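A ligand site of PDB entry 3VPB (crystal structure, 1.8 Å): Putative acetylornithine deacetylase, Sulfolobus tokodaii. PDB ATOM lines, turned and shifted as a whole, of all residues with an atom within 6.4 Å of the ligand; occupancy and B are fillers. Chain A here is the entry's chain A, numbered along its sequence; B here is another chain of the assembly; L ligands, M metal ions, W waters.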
ATOM      1  N   GLU A  13       6.023  29.710 -25.512  1.00  0.00           N
ATOM      2  CA  GLU A  13       5.273  30.419 -24.450  1.00  0.00           C
ATOM      3  C   GLU A  13       4.791  31.778 -24.961  1.00  0.00           C
ATOM      4  O   GLU A  13       3.677  32.201 -24.670  1.00  0.00           O
ATOM      5  CB  GLU A  13       6.131  30.633 -23.194  1.00  0.00           C
ATOM      6  CG  GLU A  13       6.303  29.384 -22.283  1.00  0.00           C
ATOM      7  CD  GLU A  13       7.318  28.350 -22.761  1.00  0.00           C
ATOM      8  OE1 GLU A  13       7.543  27.391 -21.989  1.00  0.00           O
ATOM      9  OE2 GLU A  13       7.877  28.451 -23.891  1.00  0.00           O
ATOM     10  N   SER A 132      20.119  30.026 -15.537  1.00  0.00           N
ATOM     11  CA  SER A 132      18.879  29.277 -15.644  1.00  0.00           C
ATOM     12  C   SER A 132      19.211  27.966 -16.344  1.00  0.00           C
ATOM     13  O   SER A 132      20.359  27.762 -16.773  1.00  0.00           O
ATOM     14  CB  SER A 132      17.853  30.084 -16.453  1.00  0.00           C
ATOM     15  OG  SER A 132      16.572  29.478 -16.459  1.00  0.00           O
ATOM     16  N   TRP A 133      18.229  27.072 -16.457  1.00  0.00           N
ATOM     17  CA  TRP A 133      18.364  25.808 -17.207  1.00  0.00           C
ATOM     18  C   TRP A 133      19.468  24.867 -16.715  1.00  0.00           C
ATOM     19  O   TRP A 133      19.932  23.990 -17.440  1.00  0.00           O
ATOM     20  CB  TRP A 133      18.571  26.069 -18.714  1.00  0.00           C
ATOM     21  CG  TRP A 133      17.497  26.854 -19.399  1.00  0.00           C
ATOM     22  CD1 TRP A 133      16.145  26.816 -19.148  1.00  0.00           C
ATOM     23  CD2 TRP A 133      17.671  27.742 -20.500  1.00  0.00           C
ATOM     24  NE1 TRP A 133      15.478  27.658 -20.009  1.00  0.00           N
ATOM     25  CE2 TRP A 133      16.388  28.211 -20.870  1.00  0.00           C
ATOM     26  CE3 TRP A 133      18.787  28.164 -21.251  1.00  0.00           C
ATOM     27  CZ2 TRP A 133      16.195  29.128 -21.916  1.00  0.00           C
ATOM     28  CZ3 TRP A 133      18.584  29.072 -22.287  1.00  0.00           C
ATOM     29  CH2 TRP A 133      17.303  29.529 -22.613  1.00  0.00           C
ATOM     30  N   ARG A 178       8.088  22.004  -9.319  1.00  0.00           N
ATOM     31  CA  ARG A 178       7.914  23.285  -9.963  1.00  0.00           C
ATOM     32  C   ARG A 178       6.474  23.744  -9.807  1.00  0.00           C
ATOM     33  O   ARG A 178       5.531  23.048 -10.190  1.00  0.00           O
ATOM     34  CB  ARG A 178       8.321  23.176 -11.445  1.00  0.00           C
ATOM     35  CG  ARG A 178       7.796  24.243 -12.397  1.00  0.00           C
ATOM     36  CD  ARG A 178       8.149  25.667 -11.985  1.00  0.00           C
ATOM     37  NE  ARG A 178       9.572  26.021 -11.994  1.00  0.00           N
ATOM     38  CZ  ARG A 178      10.227  26.491 -13.054  1.00  0.00           C
ATOM     39  NH1 ARG A 178       9.639  26.653 -14.246  1.00  0.00           N
ATOM     40  NH2 ARG A 178      11.493  26.824 -12.923  1.00  0.00           N
ATOM     41  N   ILE A 180       3.783  27.402 -10.161  1.00  0.00           N
ATOM     42  CA  ILE A 180       3.571  28.721 -10.756  1.00  0.00           C
ATOM     43  C   ILE A 180       2.516  29.447  -9.910  1.00  0.00           C
ATOM     44  O   ILE A 180       1.596  28.823  -9.443  1.00  0.00           O
ATOM     45  CB  ILE A 180       3.104  28.588 -12.202  1.00  0.00           C
ATOM     46  CG1 ILE A 180       4.293  28.136 -13.078  1.00  0.00           C
ATOM     47  CG2 ILE A 180       2.612  29.913 -12.740  1.00  0.00           C
ATOM     48  CD1 ILE A 180       3.957  27.960 -14.557  1.00  0.00           C
ATOM     49  N   TYR A 190       3.926  20.771 -10.309  1.00  0.00           N
ATOM     50  CA  TYR A 190       4.152  19.470 -10.875  1.00  0.00           C
ATOM     51  C   TYR A 190       5.576  19.038 -10.541  1.00  0.00           C
ATOM     52  O   TYR A 190       6.364  19.837 -10.005  1.00  0.00           O
ATOM     53  CB  TYR A 190       3.853  19.461 -12.373  1.00  0.00           C
ATOM     54  CG  TYR A 190       4.945  20.045 -13.249  1.00  0.00           C
ATOM     55  CD1 TYR A 190       5.094  21.426 -13.384  1.00  0.00           C
ATOM     56  CD2 TYR A 190       5.816  19.213 -13.938  1.00  0.00           C
ATOM     57  CE1 TYR A 190       6.086  21.959 -14.183  1.00  0.00           C
ATOM     58  CE2 TYR A 190       6.804  19.733 -14.733  1.00  0.00           C
ATOM     59  CZ  TYR A 190       6.928  21.111 -14.847  1.00  0.00           C
ATOM     60  OH  TYR A 190       7.919  21.624 -15.636  1.00  0.00           O
ATOM     61  N   ARG A 192       9.306  17.644 -11.759  1.00  0.00           N
ATOM     62  CA  ARG A 192      10.270  17.443 -12.855  1.00  0.00           C
ATOM     63  C   ARG A 192      11.179  16.286 -12.495  1.00  0.00           C
ATOM     64  O   ARG A 192      11.967  16.398 -11.554  1.00  0.00           O
ATOM     65  CB  ARG A 192      11.085  18.711 -13.068  1.00  0.00           C
ATOM     66  CG  ARG A 192      10.237  19.869 -13.507  1.00  0.00           C
ATOM     67  CD  ARG A 192      11.082  21.132 -13.764  1.00  0.00           C
ATOM     68  NE  ARG A 192      11.701  21.587 -12.522  1.00  0.00           N
ATOM     69  CZ  ARG A 192      12.296  22.758 -12.374  1.00  0.00           C
ATOM     70  NH1 ARG A 192      12.380  23.615 -13.399  1.00  0.00           N
ATOM     71  NH2 ARG A 192      12.797  23.086 -11.186  1.00  0.00           N
ATOM     72  N   ALA A 201      17.148  18.613 -12.590  1.00  0.00           N
ATOM     73  CA  ALA A 201      15.804  18.232 -12.958  1.00  0.00           C
ATOM     74  C   ALA A 201      15.233  19.021 -14.125  1.00  0.00           C
ATOM     75  O   ALA A 201      14.189  18.660 -14.660  1.00  0.00           O
ATOM     76  CB  ALA A 201      14.875  18.374 -11.733  1.00  0.00           C
ATOM     77  N   ASN A 202      15.925  20.088 -14.541  1.00  0.00           N
ATOM     78  CA  ASN A 202      15.371  20.996 -15.554  1.00  0.00           C
ATOM     79  C   ASN A 202      14.796  20.296 -16.767  1.00  0.00           C
ATOM     80  O   ASN A 202      15.440  19.394 -17.374  1.00  0.00           O
ATOM     81  CB  ASN A 202      16.415  22.021 -16.002  1.00  0.00           C
ATOM     82  CG  ASN A 202      17.054  22.760 -14.835  1.00  0.00           C
ATOM     83  OD1 ASN A 202      17.878  22.201 -14.117  1.00  0.00           O
ATOM     84  ND2 ASN A 202      16.677  24.030 -14.657  1.00  0.00           N
ATOM     85  N   VAL A 203      13.607  20.715 -17.176  1.00  0.00           N
ATOM     86  CA  VAL A 203      13.010  20.220 -18.435  1.00  0.00           C
ATOM     87  C   VAL A 203      13.967  20.496 -19.617  1.00  0.00           C
ATOM     88  O   VAL A 203      14.112  19.641 -20.494  1.00  0.00           O
ATOM     89  CB  VAL A 203      11.593  20.802 -18.680  1.00  0.00           C
ATOM     90  CG1 VAL A 203      11.079  20.398 -20.057  1.00  0.00           C
ATOM     91  CG2 VAL A 203      10.648  20.273 -17.588  1.00  0.00           C
ATOM     92  N   ALA A 204      14.650  21.641 -19.598  1.00  0.00           N
ATOM     93  CA  ALA A 204      15.618  21.984 -20.654  1.00  0.00           C
ATOM     94  C   ALA A 204      16.737  20.970 -20.778  1.00  0.00           C
ATOM     95  O   ALA A 204      17.378  20.881 -21.831  1.00  0.00           O
ATOM     96  CB  ALA A 204      16.204  23.408 -20.445  1.00  0.00           C
ATOM     97  N   LEU A 205      16.997  20.218 -19.694  1.00  0.00           N
ATOM     98  CA  LEU A 205      18.048  19.195 -19.660  1.00  0.00           C
ATOM     99  C   LEU A 205      17.530  17.748 -19.805  1.00  0.00           C
ATOM    100  O   LEU A 205      18.306  16.803 -19.665  1.00  0.00           O
ATOM    101  CB  LEU A 205      18.857  19.313 -18.359  1.00  0.00           C
ATOM    102  CG  LEU A 205      20.187  20.073 -18.263  1.00  0.00           C
ATOM    103  CD1 LEU A 205      20.577  20.913 -19.477  1.00  0.00           C
ATOM    104  CD2 LEU A 205      20.295  20.829 -16.932  1.00  0.00           C
ATOM    105  N   PRO A 255       8.828  32.911 -16.378  1.00  0.00           N
ATOM    106  CA  PRO A 255       8.672  31.460 -16.346  1.00  0.00           C
ATOM    107  C   PRO A 255       8.313  30.811 -17.694  1.00  0.00           C
ATOM    108  O   PRO A 255       7.554  31.354 -18.493  1.00  0.00           O
ATOM    109  CB  PRO A 255       7.601  31.246 -15.273  1.00  0.00           C
ATOM    110  CG  PRO A 255       6.889  32.490 -15.155  1.00  0.00           C
ATOM    111  CD  PRO A 255       7.812  33.618 -15.592  1.00  0.00           C
ATOM    112  N   GLU A 256       8.931  29.674 -17.958  1.00  0.00           N
ATOM    113  CA  GLU A 256       8.517  28.849 -19.052  1.00  0.00           C
ATOM    114  C   GLU A 256       7.470  27.904 -18.502  1.00  0.00           C
ATOM    115  O   GLU A 256       7.385  27.721 -17.265  1.00  0.00           O
ATOM    116  CB  GLU A 256       9.727  28.105 -19.611  1.00  0.00           C
ATOM    117  CG  GLU A 256      10.669  29.000 -20.430  1.00  0.00           C
ATOM    118  CD  GLU A 256      11.982  28.307 -20.774  1.00  0.00           C
ATOM    119  OE1 GLU A 256      12.488  27.543 -19.922  1.00  0.00           O
ATOM    120  OE2 GLU A 256      12.504  28.505 -21.888  1.00  0.00           O
ATOM    121  N   PHE A 257       6.647  27.330 -19.367  1.00  0.00           N
ATOM    122  CA  PHE A 257       5.526  26.536 -18.863  1.00  0.00           C
ATOM    123  C   PHE A 257       5.064  25.440 -19.805  1.00  0.00           C
ATOM    124  O   PHE A 257       3.978  24.896 -19.607  1.00  0.00           O
ATOM    125  CB  PHE A 257       4.327  27.411 -18.400  1.00  0.00           C
ATOM    126  CG  PHE A 257       3.932  28.505 -19.377  1.00  0.00           C
ATOM    127  CD1 PHE A 257       3.106  28.234 -20.474  1.00  0.00           C
ATOM    128  CD2 PHE A 257       4.354  29.824 -19.157  1.00  0.00           C
ATOM    129  CE1 PHE A 257       2.748  29.265 -21.368  1.00  0.00           C
ATOM    130  CE2 PHE A 257       4.009  30.858 -20.053  1.00  0.00           C
ATOM    131  CZ  PHE A 257       3.184  30.577 -21.159  1.00  0.00           C
ATOM    132  N   LYS A 258       5.910  25.046 -20.748  1.00  0.00           N
ATOM    133  CA  LYS A 258       5.570  23.919 -21.624  1.00  0.00           C
ATOM    134  C   LYS A 258       5.394  22.637 -20.818  1.00  0.00           C
ATOM    135  O   LYS A 258       4.428  21.881 -21.024  1.00  0.00           O
ATOM    136  CB  LYS A 258       6.631  23.716 -22.717  1.00  0.00           C
ATOM    137  CG  LYS A 258       6.598  24.800 -23.801  1.00  0.00           C
ATOM    138  CD  LYS A 258       7.412  24.365 -25.047  1.00  0.00           C
ATOM    139  CE  LYS A 258       8.894  24.563 -24.842  1.00  0.00           C
ATOM    140  NZ  LYS A 258       9.278  26.022 -24.817  1.00  0.00           N
ATOM    141  N   GLY A 259       6.328  22.401 -19.882  1.00  0.00           N
ATOM    142  CA  GLY A 259       6.317  21.202 -19.024  1.00  0.00           C
ATOM    143  C   GLY A 259       5.155  21.247 -18.062  1.00  0.00           C
ATOM    144  O   GLY A 259       4.453  20.227 -17.822  1.00  0.00           O
ATOM    145  N   PHE A 260       4.916  22.440 -17.517  1.00  0.00           N
ATOM    146  CA  PHE A 260       3.813  22.671 -16.592  1.00  0.00           C
ATOM    147  C   PHE A 260       2.466  22.319 -17.252  1.00  0.00           C
ATOM    148  O   PHE A 260       1.586  21.709 -16.607  1.00  0.00           O
ATOM    149  CB  PHE A 260       3.848  24.140 -16.158  1.00  0.00           C
ATOM    150  CG  PHE A 260       2.861  24.497 -15.096  1.00  0.00           C
ATOM    151  CD1 PHE A 260       3.254  24.512 -13.740  1.00  0.00           C
ATOM    152  CD2 PHE A 260       1.562  24.873 -15.430  1.00  0.00           C
ATOM    153  CE1 PHE A 260       2.322  24.878 -12.733  1.00  0.00           C
ATOM    154  CE2 PHE A 260       0.646  25.221 -14.445  1.00  0.00           C
ATOM    155  CZ  PHE A 260       1.033  25.250 -13.103  1.00  0.00           C
ATOM    156  N   MET A 261       2.313  22.703 -18.511  1.00  0.00           N
ATOM    157  CA  MET A 261       1.077  22.383 -19.256  1.00  0.00           C
ATOM    158  C   MET A 261       0.921  20.895 -19.507  1.00  0.00           C
ATOM    159  O   MET A 261      -0.163  20.361 -19.329  1.00  0.00           O
ATOM    160  CB  MET A 261       0.966  23.155 -20.574  1.00  0.00           C
ATOM    161  CG  MET A 261       0.850  24.650 -20.393  1.00  0.00           C
ATOM    162  SD  MET A 261       0.855  25.572 -21.943  1.00  0.00           S
ATOM    163  CE  MET A 261       2.093  24.750 -22.946  1.00  0.00           C
ATOM    164  N   GLY B  55      17.387  32.496 -19.881  1.00  0.00           N
ATOM    165  CA  GLY B  55      16.512  31.483 -19.334  1.00  0.00           C
ATOM    166  C   GLY B  55      15.325  32.105 -18.641  1.00  0.00           C
ATOM    167  O   GLY B  55      14.820  33.137 -19.073  1.00  0.00           O
ATOM    168  N   GLU B  56      14.874  31.436 -17.586  1.00  0.00           N
ATOM    169  CA  GLU B  56      13.751  31.922 -16.802  1.00  0.00           C
ATOM    170  C   GLU B  56      14.177  32.935 -15.753  1.00  0.00           C
ATOM    171  O   GLU B  56      13.359  33.744 -15.273  1.00  0.00           O
ATOM    172  CB  GLU B  56      13.123  30.761 -16.049  1.00  0.00           C
ATOM    173  CG  GLU B  56      12.444  29.769 -16.897  1.00  0.00           C
ATOM    174  CD  GLU B  56      11.340  29.107 -16.127  1.00  0.00           C
ATOM    175  OE1 GLU B  56      11.041  27.973 -16.440  1.00  0.00           O
ATOM    176  OE2 GLU B  56      10.775  29.737 -15.179  1.00  0.00           O
ATOM    177  OXT GLU B  56      15.348  32.913 -15.345  1.00  0.00           O
HETATM  178  N1  LIG L   1      12.835  26.462 -17.352  1.00  0.00           N
HETATM  179  C1  LIG L   1      12.074  25.284 -16.855  1.00  0.00           C
HETATM  180  C2  LIG L   1      12.913  24.018 -16.957  1.00  0.00           C
HETATM  181  O1  LIG L   1      13.781  23.866 -17.846  1.00  0.00           O
HETATM  182  C3  LIG L   1      10.763  25.115 -17.645  1.00  0.00           C
HETATM  183  C4  LIG L   1       9.809  24.094 -17.004  1.00  0.00           C
HETATM  184  C5  LIG L   1       8.464  23.990 -17.722  1.00  0.00           C
HETATM  185  O2  LIG L   1       7.426  23.855 -17.011  1.00  0.00           O
HETATM  186  O3  LIG L   1       8.460  24.048 -18.981  1.00  0.00           O
HETATM  187  O4  LIG L   1      12.682  23.105 -16.148  1.00  0.00           O
HETATM  188 MG    MG M   1      15.659  25.870 -11.405  1.00  0.00          MG
HETATM  189  O   HOH W   1      10.185  23.803 -21.009  1.00  0.00           O
HETATM  190  O   HOH W   2       6.993  25.897 -15.255  1.00  0.00           O
HETATM  191  O   HOH W   3      12.842  24.513 -20.771  1.00  0.00           O
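CD1 of Trp 133 touches N1 of the ligand, 3.8 Å away.
NH1 of Arg 178 touches C4 of the ligand, 3.8 Å away.
Asn 202 touches the ligand.
Phe 257 touches the ligand (C to O3, 3.8 Å).
Hydrophobic or aromatic side chains within 4 Å of the ligand: Trp 133, Tyr 190, Val 203, Ala 204 and Phe 260.
13 residues have an atom within 4 Å of the ligand: Trp 133, Arg 178, Tyr 190, Arg 192, Asn 202, Val 203, Ala 204, Glu 256, Phe 257, Lys 258, Gly 259, Phe 260 and Glu 56 of chain B.
The side-chain carboxylate (OE1) of Glu 56 of chain B lies close to the backbone NH (N) of Glu 256 (3.1 Å).
The backbone NH (N) of Phe 257 is in hydrogen-bond range of the side-chain carboxylate (OE1) of Glu 13, 2.8 Å away.
The side-chain amino group (NZ) of Lys 258 is in salt-bridge range of the side-chain carboxylate (OE2) of Glu 13 (3.0 Å).
The indole nitrogen (NE1) of Trp 133 sits at hydrogen-bond distance from the side-chain carboxylate (OE1) of Glu 256, at 3.0 Å.
OE1 of Glu 56 of chain B is in salt-bridge range of NH1 of Arg 178 (2.9 Å).
N of Tyr 190 sits at hydrogen-bond distance from O of Arg 178.
The backbone NH (N) of Glu 56 of chain B sits at hydrogen-bond distance from the side-chain hydroxyl (OG) of Ser 132, 2.8 Å away.
Water W2 lies within hydrogen-bond range of O2 of the ligand (2.7 Å), O of Glu 256 (2.7 Å) and NH1 of Arg 178 (2.9 Å).
Water W3 bridges an oxygen (O1) of the ligand (3.1 Å) and the side-chain carboxylate (OE1) of Glu 256 (3.2 Å).
The backbone NH of Lys 258 is in hydrogen-bond range of an oxygen (O3) of the ligand, at 3.3 Å.
An oxygen (O4) of the ligand sits at hydrogen-bond distance from the backbone NH (N) of Val 203.
A nitrogen (N1) of the ligand is in salt-bridge range of the side-chain carboxylate (OE1) of Glu 56 of chain B, at 2.5 Å.
The guanidinium group of Arg 192 is in salt-bridge range of an oxygen (O4) of the ligand (2.8 Å).
O3 of the ligand sits at hydrogen-bond distance from N of Gly 259.
The backbone NH (N) of Ala 204 lies within hydrogen-bond range of an oxygen (O1) of the ligand (3.0 Å).
N of Phe 260 lies within hydrogen-bond range of O2 of the ligand (2.9 Å).
The side-chain carboxylate (OE1) of Glu 256 is in salt-bridge range of a nitrogen (N1) of the ligand, at 2.8 Å.
The side-chain hydroxyl (OH) of Tyr 190 sits at hydrogen-bond distance from an oxygen (O2) of the ligand, at 2.7 Å.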
